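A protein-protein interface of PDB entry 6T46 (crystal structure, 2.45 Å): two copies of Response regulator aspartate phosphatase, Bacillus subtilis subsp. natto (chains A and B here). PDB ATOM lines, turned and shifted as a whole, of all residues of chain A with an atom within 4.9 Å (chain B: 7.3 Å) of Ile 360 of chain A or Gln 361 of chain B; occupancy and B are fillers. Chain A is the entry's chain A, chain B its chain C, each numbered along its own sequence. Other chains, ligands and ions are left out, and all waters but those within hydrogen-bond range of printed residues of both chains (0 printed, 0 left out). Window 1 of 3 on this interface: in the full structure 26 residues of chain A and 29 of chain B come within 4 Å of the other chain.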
ATOM      1  N   ILE A 146      -8.796 -16.115 -10.283  1.00  0.00           N
ATOM      2  CA  ILE A 146      -7.866 -15.075  -9.880  1.00  0.00           C
ATOM      3  C   ILE A 146      -7.872 -14.905  -8.361  1.00  0.00           C
ATOM      4  O   ILE A 146      -7.566 -13.828  -7.854  1.00  0.00           O
ATOM      5  CB  ILE A 146      -8.116 -13.740 -10.597  1.00  0.00           C
ATOM      6  CG1 ILE A 146      -9.582 -13.355 -10.628  1.00  0.00           C
ATOM      7  CG2 ILE A 146      -7.681 -13.850 -12.044  1.00  0.00           C
ATOM      8  CD1 ILE A 146      -9.773 -11.983 -11.220  1.00  0.00           C
ATOM      9  N   ASP A 147      -8.327 -15.920  -7.635  1.00  0.00           N
ATOM     10  CA  ASP A 147      -8.118 -16.004  -6.188  1.00  0.00           C
ATOM     11  C   ASP A 147      -8.881 -14.932  -5.407  1.00  0.00           C
ATOM     12  O   ASP A 147      -8.390 -14.426  -4.402  1.00  0.00           O
ATOM     13  CB  ASP A 147      -6.622 -15.953  -5.875  1.00  0.00           C
ATOM     14  CG  ASP A 147      -5.890 -17.229  -6.330  1.00  0.00           C
ATOM     15  OD1 ASP A 147      -5.955 -18.268  -5.611  1.00  0.00           O
ATOM     16  OD2 ASP A 147      -5.282 -17.186  -7.440  1.00  0.00           O
ATOM     17  N   HIS A 149     -11.667 -15.231  -3.358  1.00  0.00           N
ATOM     18  CA  HIS A 149     -12.464 -16.342  -2.836  1.00  0.00           C
ATOM     19  C   HIS A 149     -13.795 -15.914  -2.214  1.00  0.00           C
ATOM     20  O   HIS A 149     -14.816 -16.576  -2.433  1.00  0.00           O
ATOM     21  CB  HIS A 149     -11.639 -17.143  -1.849  1.00  0.00           C
ATOM     22  CG  HIS A 149     -10.373 -17.641  -2.445  1.00  0.00           C
ATOM     23  ND1 HIS A 149     -10.357 -18.465  -3.555  1.00  0.00           N
ATOM     24  CD2 HIS A 149      -9.081 -17.458  -2.086  1.00  0.00           C
ATOM     25  CE1 HIS A 149      -9.103 -18.756  -3.861  1.00  0.00           C
ATOM     26  NE2 HIS A 149      -8.309 -18.163  -2.982  1.00  0.00           N
ATOM     27  N   ASP A 186      -8.902 -23.496  -0.941  1.00  0.00           N
ATOM     28  CA  ASP A 186      -7.853 -22.530  -1.233  1.00  0.00           C
ATOM     29  C   ASP A 186      -7.714 -21.537  -0.096  1.00  0.00           C
ATOM     30  O   ASP A 186      -6.605 -21.125   0.256  1.00  0.00           O
ATOM     31  CB  ASP A 186      -8.185 -21.773  -2.510  1.00  0.00           C
ATOM     32  CG  ASP A 186      -7.918 -22.571  -3.758  1.00  0.00           C
ATOM     33  OD1 ASP A 186      -7.527 -23.755  -3.693  1.00  0.00           O
ATOM     34  OD2 ASP A 186      -8.114 -21.986  -4.831  1.00  0.00           O
ATOM     35  N   MET A 187      -8.830 -21.161   0.512  1.00  0.00           N
ATOM     36  CA  MET A 187      -8.774 -20.291   1.672  1.00  0.00           C
ATOM     37  C   MET A 187      -8.168 -20.979   2.872  1.00  0.00           C
ATOM     38  O   MET A 187      -7.789 -20.299   3.838  1.00  0.00           O
ATOM     39  CB  MET A 187     -10.169 -19.833   2.053  1.00  0.00           C
ATOM     40  CG  MET A 187     -10.720 -18.827   1.112  1.00  0.00           C
ATOM     41  SD  MET A 187     -12.385 -18.482   1.623  1.00  0.00           S
ATOM     42  CE  MET A 187     -13.190 -19.584   0.490  1.00  0.00           C
ATOM     43  N   TRP A 323       1.256 -18.489  -9.139  1.00  0.00           N
ATOM     44  CA  TRP A 323       1.785 -18.104  -7.834  1.00  0.00           C
ATOM     45  C   TRP A 323       1.196 -18.882  -6.662  1.00  0.00           C
ATOM     46  O   TRP A 323       1.973 -19.266  -5.770  1.00  0.00           O
ATOM     47  CB  TRP A 323       1.645 -16.601  -7.650  1.00  0.00           C
ATOM     48  CG  TRP A 323       2.485 -15.896  -8.607  1.00  0.00           C
ATOM     49  CD1 TRP A 323       2.077 -15.152  -9.669  1.00  0.00           C
ATOM     50  CD2 TRP A 323       3.901 -15.848  -8.598  1.00  0.00           C
ATOM     51  NE1 TRP A 323       3.163 -14.637 -10.328  1.00  0.00           N
ATOM     52  CE2 TRP A 323       4.299 -15.056  -9.688  1.00  0.00           C
ATOM     53  CE3 TRP A 323       4.875 -16.397  -7.774  1.00  0.00           C
ATOM     54  CZ2 TRP A 323       5.639 -14.803  -9.981  1.00  0.00           C
ATOM     55  CZ3 TRP A 323       6.214 -16.148  -8.067  1.00  0.00           C
ATOM     56  CH2 TRP A 323       6.580 -15.351  -9.161  1.00  0.00           C
ATOM     57  N   PRO A 324      -0.109 -19.156  -6.590  1.00  0.00           N
ATOM     58  CA  PRO A 324      -0.579 -20.038  -5.513  1.00  0.00           C
ATOM     59  C   PRO A 324       0.189 -21.338  -5.441  1.00  0.00           C
ATOM     60  O   PRO A 324       0.617 -21.723  -4.345  1.00  0.00           O
ATOM     61  CB  PRO A 324      -2.053 -20.243  -5.860  1.00  0.00           C
ATOM     62  CG  PRO A 324      -2.436 -18.940  -6.464  1.00  0.00           C
ATOM     63  CD  PRO A 324      -1.234 -18.525  -7.290  1.00  0.00           C
ATOM     64  N   ALA A 356       6.123 -15.444  -3.453  1.00  0.00           N
ATOM     65  CA  ALA A 356       4.988 -15.933  -4.237  1.00  0.00           C
ATOM     66  C   ALA A 356       3.661 -15.536  -3.616  1.00  0.00           C
ATOM     67  O   ALA A 356       2.740 -15.142  -4.333  1.00  0.00           O
ATOM     68  CB  ALA A 356       5.034 -17.442  -4.392  1.00  0.00           C
ATOM     69  N   LYS A 357       3.516 -15.660  -2.292  1.00  0.00           N
ATOM     70  CA  LYS A 357       2.270 -15.203  -1.686  1.00  0.00           C
ATOM     71  C   LYS A 357       2.011 -13.747  -2.050  1.00  0.00           C
ATOM     72  O   LYS A 357       0.879 -13.367  -2.352  1.00  0.00           O
ATOM     73  CB  LYS A 357       2.296 -15.383  -0.168  1.00  0.00           C
ATOM     74  CG  LYS A 357       2.212 -16.840   0.264  1.00  0.00           C
ATOM     75  CD  LYS A 357       0.844 -17.418  -0.042  1.00  0.00           C
ATOM     76  CE  LYS A 357       0.532 -18.659   0.788  1.00  0.00           C
ATOM     77  NZ  LYS A 357      -0.516 -19.494   0.096  1.00  0.00           N
ATOM     78  N   GLU A 358       3.068 -12.945  -2.131  1.00  0.00           N
ATOM     79  CA  GLU A 358       2.891 -11.538  -2.451  1.00  0.00           C
ATOM     80  C   GLU A 358       2.408 -11.337  -3.873  1.00  0.00           C
ATOM     81  O   GLU A 358       1.826 -10.298  -4.177  1.00  0.00           O
ATOM     82  CB  GLU A 358       4.208 -10.784  -2.279  1.00  0.00           C
ATOM     83  CG  GLU A 358       4.821 -10.796  -0.879  1.00  0.00           C
ATOM     84  CD  GLU A 358       5.864  -9.704  -0.725  1.00  0.00           C
ATOM     85  OE1 GLU A 358       6.796  -9.650  -1.561  1.00  0.00           O
ATOM     86  OE2 GLU A 358       5.787  -8.926   0.251  1.00  0.00           O
ATOM     87  N   GLN A 359       2.704 -12.256  -4.777  1.00  0.00           N
ATOM     88  CA  GLN A 359       2.272 -12.080  -6.161  1.00  0.00           C
ATOM     89  C   GLN A 359       0.824 -12.477  -6.394  1.00  0.00           C
ATOM     90  O   GLN A 359       0.268 -12.108  -7.435  1.00  0.00           O
ATOM     91  CB  GLN A 359       3.142 -12.902  -7.104  1.00  0.00           C
ATOM     92  CG  GLN A 359       4.628 -12.646  -6.954  1.00  0.00           C
ATOM     93  CD  GLN A 359       4.997 -11.188  -7.029  1.00  0.00           C
ATOM     94  OE1 GLN A 359       4.904 -10.579  -8.092  1.00  0.00           O
ATOM     95  NE2 GLN A 359       5.374 -10.608  -5.894  1.00  0.00           N
ATOM     96  N   ILE A 360       0.205 -13.244  -5.485  1.00  0.00           N
ATOM     97  CA  ILE A 360      -1.041 -13.935  -5.843  1.00  0.00           C
ATOM     98  C   ILE A 360      -2.093 -12.975  -6.367  1.00  0.00           C
ATOM     99  O   ILE A 360      -2.866 -13.321  -7.271  1.00  0.00           O
ATOM    100  CB  ILE A 360      -1.591 -14.754  -4.658  1.00  0.00           C
ATOM    101  CG1 ILE A 360      -0.650 -15.886  -4.265  1.00  0.00           C
ATOM    102  CG2 ILE A 360      -2.910 -15.396  -5.038  1.00  0.00           C
ATOM    103  CD1 ILE A 360      -1.206 -16.703  -3.115  1.00  0.00           C
ATOM    104  N   GLN A 361      -2.194 -11.791  -5.769  1.00  0.00           N
ATOM    105  CA  GLN A 361      -3.193 -10.791  -6.139  1.00  0.00           C
ATOM    106  C   GLN A 361      -2.631  -9.667  -6.984  1.00  0.00           C
ATOM    107  O   GLN A 361      -3.306  -8.661  -7.171  1.00  0.00           O
ATOM    108  CB  GLN A 361      -3.862 -10.240  -4.891  1.00  0.00           C
ATOM    109  CG  GLN A 361      -5.294 -10.687  -4.695  1.00  0.00           C
ATOM    110  CD  GLN A 361      -5.739 -10.439  -3.265  1.00  0.00           C
ATOM    111  OE1 GLN A 361      -4.938 -10.551  -2.335  1.00  0.00           O
ATOM    112  NE2 GLN A 361      -6.993 -10.053  -3.085  1.00  0.00           N
ATOM    113  N   ARG A 362      -1.402  -9.794  -7.465  1.00  0.00           N
ATOM    114  CA  ARG A 362      -0.843  -8.759  -8.312  1.00  0.00           C
ATOM    115  C   ARG A 362      -1.476  -8.736  -9.699  1.00  0.00           C
ATOM    116  O   ARG A 362      -1.308  -7.736 -10.397  1.00  0.00           O
ATOM    117  CB  ARG A 362       0.665  -8.938  -8.355  1.00  0.00           C
ATOM    118  CG  ARG A 362       1.433  -7.835  -9.037  1.00  0.00           C
ATOM    119  CD  ARG A 362       2.909  -8.011  -8.764  1.00  0.00           C
ATOM    120  NE  ARG A 362       3.671  -6.830  -9.150  1.00  0.00           N
ATOM    121  CZ  ARG A 362       5.000  -6.755  -9.105  1.00  0.00           C
ATOM    122  NH1 ARG A 362       5.707  -7.789  -8.664  1.00  0.00           N
ATOM    123  NH2 ARG A 362       5.619  -5.634  -9.476  1.00  0.00           N
ATOM    124  N   ILE A 363      -2.177  -9.806 -10.103  1.00  0.00           N
ATOM    125  CA  ILE A 363      -3.180  -9.881 -11.181  1.00  0.00           C
ATOM    126  C   ILE A 363      -2.704 -10.387 -12.533  1.00  0.00           C
ATOM    127  O   ILE A 363      -3.498 -11.012 -13.237  1.00  0.00           O
ATOM    128  CB  ILE A 363      -3.978  -8.568 -11.369  1.00  0.00           C
ATOM    129  CG1 ILE A 363      -5.172  -8.880 -12.272  1.00  0.00           C
ATOM    130  CG2 ILE A 363      -3.214  -7.551 -12.142  1.00  0.00           C
ATOM    131  CD1 ILE A 363      -5.887 -10.201 -11.918  1.00  0.00           C
ATOM    132  N   ILE B 146     -11.124  -6.522   3.983  1.00  0.00           N
ATOM    133  CA  ILE B 146     -10.790  -7.926   4.100  1.00  0.00           C
ATOM    134  C   ILE B 146      -9.888  -8.370   2.956  1.00  0.00           C
ATOM    135  O   ILE B 146      -9.868  -9.554   2.614  1.00  0.00           O
ATOM    136  CB  ILE B 146     -12.031  -8.809   4.206  1.00  0.00           C
ATOM    137  CG1 ILE B 146     -12.917  -8.537   3.021  1.00  0.00           C
ATOM    138  CG2 ILE B 146     -12.747  -8.495   5.497  1.00  0.00           C
ATOM    139  CD1 ILE B 146     -14.054  -9.461   2.938  1.00  0.00           C
ATOM    140  N   ASP B 147      -9.237  -7.422   2.287  1.00  0.00           N
ATOM    141  CA  ASP B 147      -8.128  -7.698   1.371  1.00  0.00           C
ATOM    142  C   ASP B 147      -8.556  -8.494   0.135  1.00  0.00           C
ATOM    143  O   ASP B 147      -7.778  -9.267  -0.421  1.00  0.00           O
ATOM    144  CB  ASP B 147      -7.015  -8.399   2.128  1.00  0.00           C
ATOM    145  CG  ASP B 147      -6.505  -7.536   3.264  1.00  0.00           C
ATOM    146  OD1 ASP B 147      -7.037  -7.709   4.384  1.00  0.00           O
ATOM    147  OD2 ASP B 147      -5.640  -6.644   3.044  1.00  0.00           O
ATOM    148  N   GLN B 148      -9.789  -8.278  -0.307  1.00  0.00           N
ATOM    149  CA  GLN B 148     -10.280  -8.792  -1.577  1.00  0.00           C
ATOM    150  C   GLN B 148     -10.150  -7.690  -2.630  1.00  0.00           C
ATOM    151  O   GLN B 148     -11.136  -7.101  -3.083  1.00  0.00           O
ATOM    152  CB  GLN B 148     -11.718  -9.227  -1.405  1.00  0.00           C
ATOM    153  CG  GLN B 148     -11.821 -10.350  -0.411  1.00  0.00           C
ATOM    154  CD  GLN B 148     -11.753 -11.694  -1.046  1.00  0.00           C
ATOM    155  OE1 GLN B 148     -12.381 -11.961  -2.102  1.00  0.00           O
ATOM    156  NE2 GLN B 148     -10.976 -12.557  -0.434  1.00  0.00           N
ATOM    157  N   LEU B 150      -9.149  -7.346  -5.855  1.00  0.00           N
ATOM    158  CA  LEU B 150      -9.643  -7.297  -7.231  1.00  0.00           C
ATOM    159  C   LEU B 150     -11.069  -6.806  -7.298  1.00  0.00           C
ATOM    160  O   LEU B 150     -11.377  -5.910  -8.078  1.00  0.00           O
ATOM    161  CB  LEU B 150      -9.564  -8.651  -7.888  1.00  0.00           C
ATOM    162  CG  LEU B 150      -8.267  -8.712  -8.657  1.00  0.00           C
ATOM    163  CD1 LEU B 150      -8.428  -7.851  -9.906  1.00  0.00           C
ATOM    164  CD2 LEU B 150      -7.135  -8.244  -7.743  1.00  0.00           C
ATOM    165  N   MET B 187      -2.157  -4.514  -3.416  1.00  0.00           N
ATOM    166  CA  MET B 187      -1.874  -5.574  -4.391  1.00  0.00           C
ATOM    167  C   MET B 187      -0.394  -5.655  -4.750  1.00  0.00           C
ATOM    168  O   MET B 187       0.016  -6.613  -5.435  1.00  0.00           O
ATOM    169  CB  MET B 187      -2.649  -5.354  -5.689  1.00  0.00           C
ATOM    170  CG  MET B 187      -4.116  -5.517  -5.577  1.00  0.00           C
ATOM    171  SD  MET B 187      -4.941  -4.744  -6.965  1.00  0.00           S
ATOM    172  CE  MET B 187      -4.679  -6.005  -8.147  1.00  0.00           C
ATOM    173  N   TRP B 323      -3.687  -9.045  10.175  1.00  0.00           N
ATOM    174  CA  TRP B 323      -2.760  -9.948   9.504  1.00  0.00           C
ATOM    175  C   TRP B 323      -1.975  -9.252   8.406  1.00  0.00           C
ATOM    176  O   TRP B 323      -0.752  -9.477   8.328  1.00  0.00           O
ATOM    177  CB  TRP B 323      -3.508 -11.167   8.963  1.00  0.00           C
ATOM    178  CG  TRP B 323      -4.145 -11.941  10.044  1.00  0.00           C
ATOM    179  CD1 TRP B 323      -5.484 -12.051  10.294  1.00  0.00           C
ATOM    180  CD2 TRP B 323      -3.484 -12.701  11.063  1.00  0.00           C
ATOM    181  NE1 TRP B 323      -5.697 -12.855  11.397  1.00  0.00           N
ATOM    182  CE2 TRP B 323      -4.486 -13.265  11.884  1.00  0.00           C
ATOM    183  CE3 TRP B 323      -2.145 -12.974  11.349  1.00  0.00           C
ATOM    184  CZ2 TRP B 323      -4.192 -14.067  12.966  1.00  0.00           C
ATOM    185  CZ3 TRP B 323      -1.861 -13.775  12.422  1.00  0.00           C
ATOM    186  CH2 TRP B 323      -2.879 -14.308  13.224  1.00  0.00           C
ATOM    187  N   ALA B 356       1.183 -15.334   8.545  1.00  0.00           N
ATOM    188  CA  ALA B 356       0.259 -14.206   8.469  1.00  0.00           C
ATOM    189  C   ALA B 356      -0.381 -14.130   7.096  1.00  0.00           C
ATOM    190  O   ALA B 356      -1.593 -13.934   6.982  1.00  0.00           O
ATOM    191  CB  ALA B 356       0.973 -12.893   8.781  1.00  0.00           C
ATOM    192  N   LYS B 357       0.416 -14.282   6.033  1.00  0.00           N
ATOM    193  CA  LYS B 357      -0.162 -14.239   4.695  1.00  0.00           C
ATOM    194  C   LYS B 357      -1.261 -15.266   4.563  1.00  0.00           C
ATOM    195  O   LYS B 357      -2.295 -15.011   3.937  1.00  0.00           O
ATOM    196  CB  LYS B 357       0.888 -14.493   3.628  1.00  0.00           C
ATOM    197  CG  LYS B 357       1.862 -13.367   3.500  1.00  0.00           C
ATOM    198  CD  LYS B 357       1.180 -12.165   2.944  1.00  0.00           C
ATOM    199  CE  LYS B 357       2.173 -11.214   2.303  1.00  0.00           C
ATOM    200  NZ  LYS B 357       2.486 -10.136   3.288  1.00  0.00           N
ATOM    201  N   GLU B 358      -1.079 -16.422   5.179  1.00  0.00           N
ATOM    202  CA  GLU B 358      -2.102 -17.440   5.063  1.00  0.00           C
ATOM    203  C   GLU B 358      -3.373 -17.057   5.798  1.00  0.00           C
ATOM    204  O   GLU B 358      -4.456 -17.466   5.378  1.00  0.00           O
ATOM    205  CB  GLU B 358      -1.534 -18.732   5.579  1.00  0.00           C
ATOM    206  CG  GLU B 358      -0.345 -19.100   4.773  1.00  0.00           C
ATOM    207  CD  GLU B 358       0.043 -20.525   4.991  1.00  0.00           C
ATOM    208  OE1 GLU B 358       0.285 -20.877   6.172  1.00  0.00           O
ATOM    209  OE2 GLU B 358       0.117 -21.287   3.992  1.00  0.00           O
ATOM    210  N   GLN B 359      -3.285 -16.251   6.864  1.00  0.00           N
ATOM    211  CA  GLN B 359      -4.517 -15.851   7.538  1.00  0.00           C
ATOM    212  C   GLN B 359      -5.258 -14.777   6.765  1.00  0.00           C
ATOM    213  O   GLN B 359      -6.482 -14.656   6.901  1.00  0.00           O
ATOM    214  CB  GLN B 359      -4.230 -15.338   8.946  1.00  0.00           C
ATOM    215  CG  GLN B 359      -3.560 -16.325   9.858  1.00  0.00           C
ATOM    216  CD  GLN B 359      -4.264 -17.663   9.846  1.00  0.00           C
ATOM    217  OE1 GLN B 359      -5.409 -17.779  10.300  1.00  0.00           O
ATOM    218  NE2 GLN B 359      -3.591 -18.680   9.318  1.00  0.00           N
ATOM    219  N   ILE B 360      -4.548 -13.978   5.968  1.00  0.00           N
ATOM    220  CA  ILE B 360      -5.236 -12.988   5.147  1.00  0.00           C
ATOM    221  C   ILE B 360      -6.195 -13.693   4.207  1.00  0.00           C
ATOM    222  O   ILE B 360      -7.316 -13.232   3.968  1.00  0.00           O
ATOM    223  CB  ILE B 360      -4.244 -12.124   4.363  1.00  0.00           C
ATOM    224  CG1 ILE B 360      -3.360 -11.321   5.317  1.00  0.00           C
ATOM    225  CG2 ILE B 360      -4.996 -11.194   3.471  1.00  0.00           C
ATOM    226  CD1 ILE B 360      -2.359 -10.476   4.570  1.00  0.00           C
ATOM    227  N   GLN B 361      -5.803 -14.862   3.717  1.00  0.00           N
ATOM    228  CA  GLN B 361      -6.626 -15.515   2.720  1.00  0.00           C
ATOM    229  C   GLN B 361      -7.728 -16.357   3.329  1.00  0.00           C
ATOM    230  O   GLN B 361      -8.746 -16.575   2.662  1.00  0.00           O
ATOM    231  CB  GLN B 361      -5.733 -16.418   1.878  1.00  0.00           C
ATOM    232  CG  GLN B 361      -5.575 -15.954   0.468  1.00  0.00           C
ATOM    233  CD  GLN B 361      -4.609 -16.809  -0.287  1.00  0.00           C
ATOM    234  OE1 GLN B 361      -3.652 -17.340   0.291  1.00  0.00           O
ATOM    235  NE2 GLN B 361      -4.867 -16.988  -1.588  1.00  0.00           N
ATOM    236  N   ARG B 362      -7.607 -16.704   4.613  1.00  0.00           N
ATOM    237  CA  ARG B 362      -8.644 -17.448   5.318  1.00  0.00           C
ATOM    238  C   ARG B 362      -9.830 -16.584   5.713  1.00  0.00           C
ATOM    239  O   ARG B 362     -10.950 -17.101   5.828  1.00  0.00           O
ATOM    240  CB  ARG B 362      -8.046 -18.048   6.586  1.00  0.00           C
ATOM    241  CG  ARG B 362      -8.940 -18.955   7.402  1.00  0.00           C
ATOM    242  CD  ARG B 362      -8.124 -19.555   8.560  1.00  0.00           C
ATOM    243  NE  ARG B 362      -8.318 -20.994   8.759  1.00  0.00           N
ATOM    244  CZ  ARG B 362      -9.433 -21.535   9.249  1.00  0.00           C
ATOM    245  NH1 ARG B 362     -10.467 -20.746   9.575  1.00  0.00           N
ATOM    246  NH2 ARG B 362      -9.525 -22.861   9.398  1.00  0.00           N
ATOM    247  N   ILE B 363      -9.624 -15.272   5.829  1.00  0.00           N
ATOM    248  CA  ILE B 363     -10.653 -14.324   6.248  1.00  0.00           C
ATOM    249  C   ILE B 363     -10.955 -14.708   7.694  1.00  0.00           C
ATOM    250  O   ILE B 363     -11.356 -15.842   7.981  1.00  0.00           O
ATOM    251  CB  ILE B 363     -11.902 -14.356   5.348  1.00  0.00           C
ATOM    252  CG1 ILE B 363     -11.670 -13.499   4.122  1.00  0.00           C
ATOM    253  CG2 ILE B 363     -13.107 -13.760   6.079  1.00  0.00           C
ATOM    254  CD1 ILE B 363     -12.713 -13.679   3.098  1.00  0.00           C
ATOM    255  N   THR B 364     -10.737 -13.787   8.624  1.00  0.00           N
ATOM    256  CA  THR B 364     -10.912 -14.142  10.028  1.00  0.00           C
ATOM    257  C   THR B 364     -12.350 -13.882  10.479  1.00  0.00           C
ATOM    258  O   THR B 364     -12.599 -13.288  11.522  1.00  0.00           O
ATOM    259  CB  THR B 364      -9.897 -13.389  10.881  1.00  0.00           C
ATOM    260  OG1 THR B 364      -8.588 -13.731  10.430  1.00  0.00           O
ATOM    261  CG2 THR B 364      -9.952 -13.852  12.337  1.00  0.00           C
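The side-chain amide nitrogen (NE2) of Gln 361 of chain A sits at hydrogen-bond distance from the backbone carbonyl oxygen (O) of Asp 147 of chain B, 2.9 Å away.
The guanidinium group of Arg 362 of chain A is in hydrogen-bond range of the side-chain amide oxygen of Gln 359 of chain A (3.0 Å).
Among the printed residues, pairs that only touch across the chains: Gln 361 of chain A with Met 187 of chain B (3.1 Å), Met 187 of chain A with Arg 362 of chain B (3.3 Å), Met 187 of chain A with Gln 361 of chain B (3.4 Å), His 149 of chain A with Gln 148 of chain B (3.6 Å), Arg 362 of chain A with Met 187 of chain B (3.7 Å), Lys 357 of chain A with Gln 361 of chain B (3.8 Å), Gln 361 of chain A with Gln 148 of chain B (3.8 Å), Gln 361 of chain A with Leu 150 of chain B (3.9 Å), His 149 of chain A with Gln 361 of chain B (3.9 Å) and Ile 360 of chain A with Gln 361 of chain B (3.98 Å).
Of the printed residues of chain B, Ile 360 of chain A touches Gln 361 (3.98 Å). Printed residues of chain A within 4 Å of Gln 361 of chain B: His 149 (3.9 Å), Met 187 (3.4 Å), Lys 357 (3.8 Å) and Ile 360 (3.98 Å). Printed residues of chain A within 4 Å of Asp 147 of chain B: Gln 361 (2.9 Å). Printed residues of chain A within 4 Å of Arg 362 of chain B: Met 187. Printed residues of chain B within 4 Å of Lys 357 of chain A: Gln 361 (3.8 Å). The nearest printed residue of chain B that does not touch Ile 360 of chain A is Met 187 of chain B (6.6 Å). The nearest residue of chain A that does not touch Gln 361 of chain B is Asp 147 of chain A (4.4 Å). The nearest printed residue of chain A that does not touch Met 187 of chain B is Ile 363 of chain A (4.2 Å).
Of the 15 printed residues of chain A, 6 touch a printed residue of chain B. Hydrophobic or aromatic side chains of chain A within 4 Å of the printed part of chain B: His 149, Met 187 and Ile 360. Among the printed residues, no Asp or Glu carboxylate lies within 4 Å of a Lys or Arg side-chain nitrogen of the other chain.
Met 187 of chain A touches Gln 361 of chain B, and with the chains exchanged Gln 361 of chain A touches Met 187 of chain B. Lys 357 of chain A touches Gln 361 of chain B, but with the chains exchanged Gln 361 of chain A does not touch Lys 357 of chain B (8.1 Å). Ile 360 of chain A touches Gln 361 of chain B, but with the chains exchanged Gln 361 of chain A does not touch Ile 360 of chain B (5.8 Å). Gln 361 of chain A touches Asp 147 of chain B, but with the chains exchanged Asp 147 of chain A does not touch Gln 361 of chain B (4.4 Å). Of the 11 pairs that touch across the chains among the printed residues, 4 have their exchanged pair printed and touching as well.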
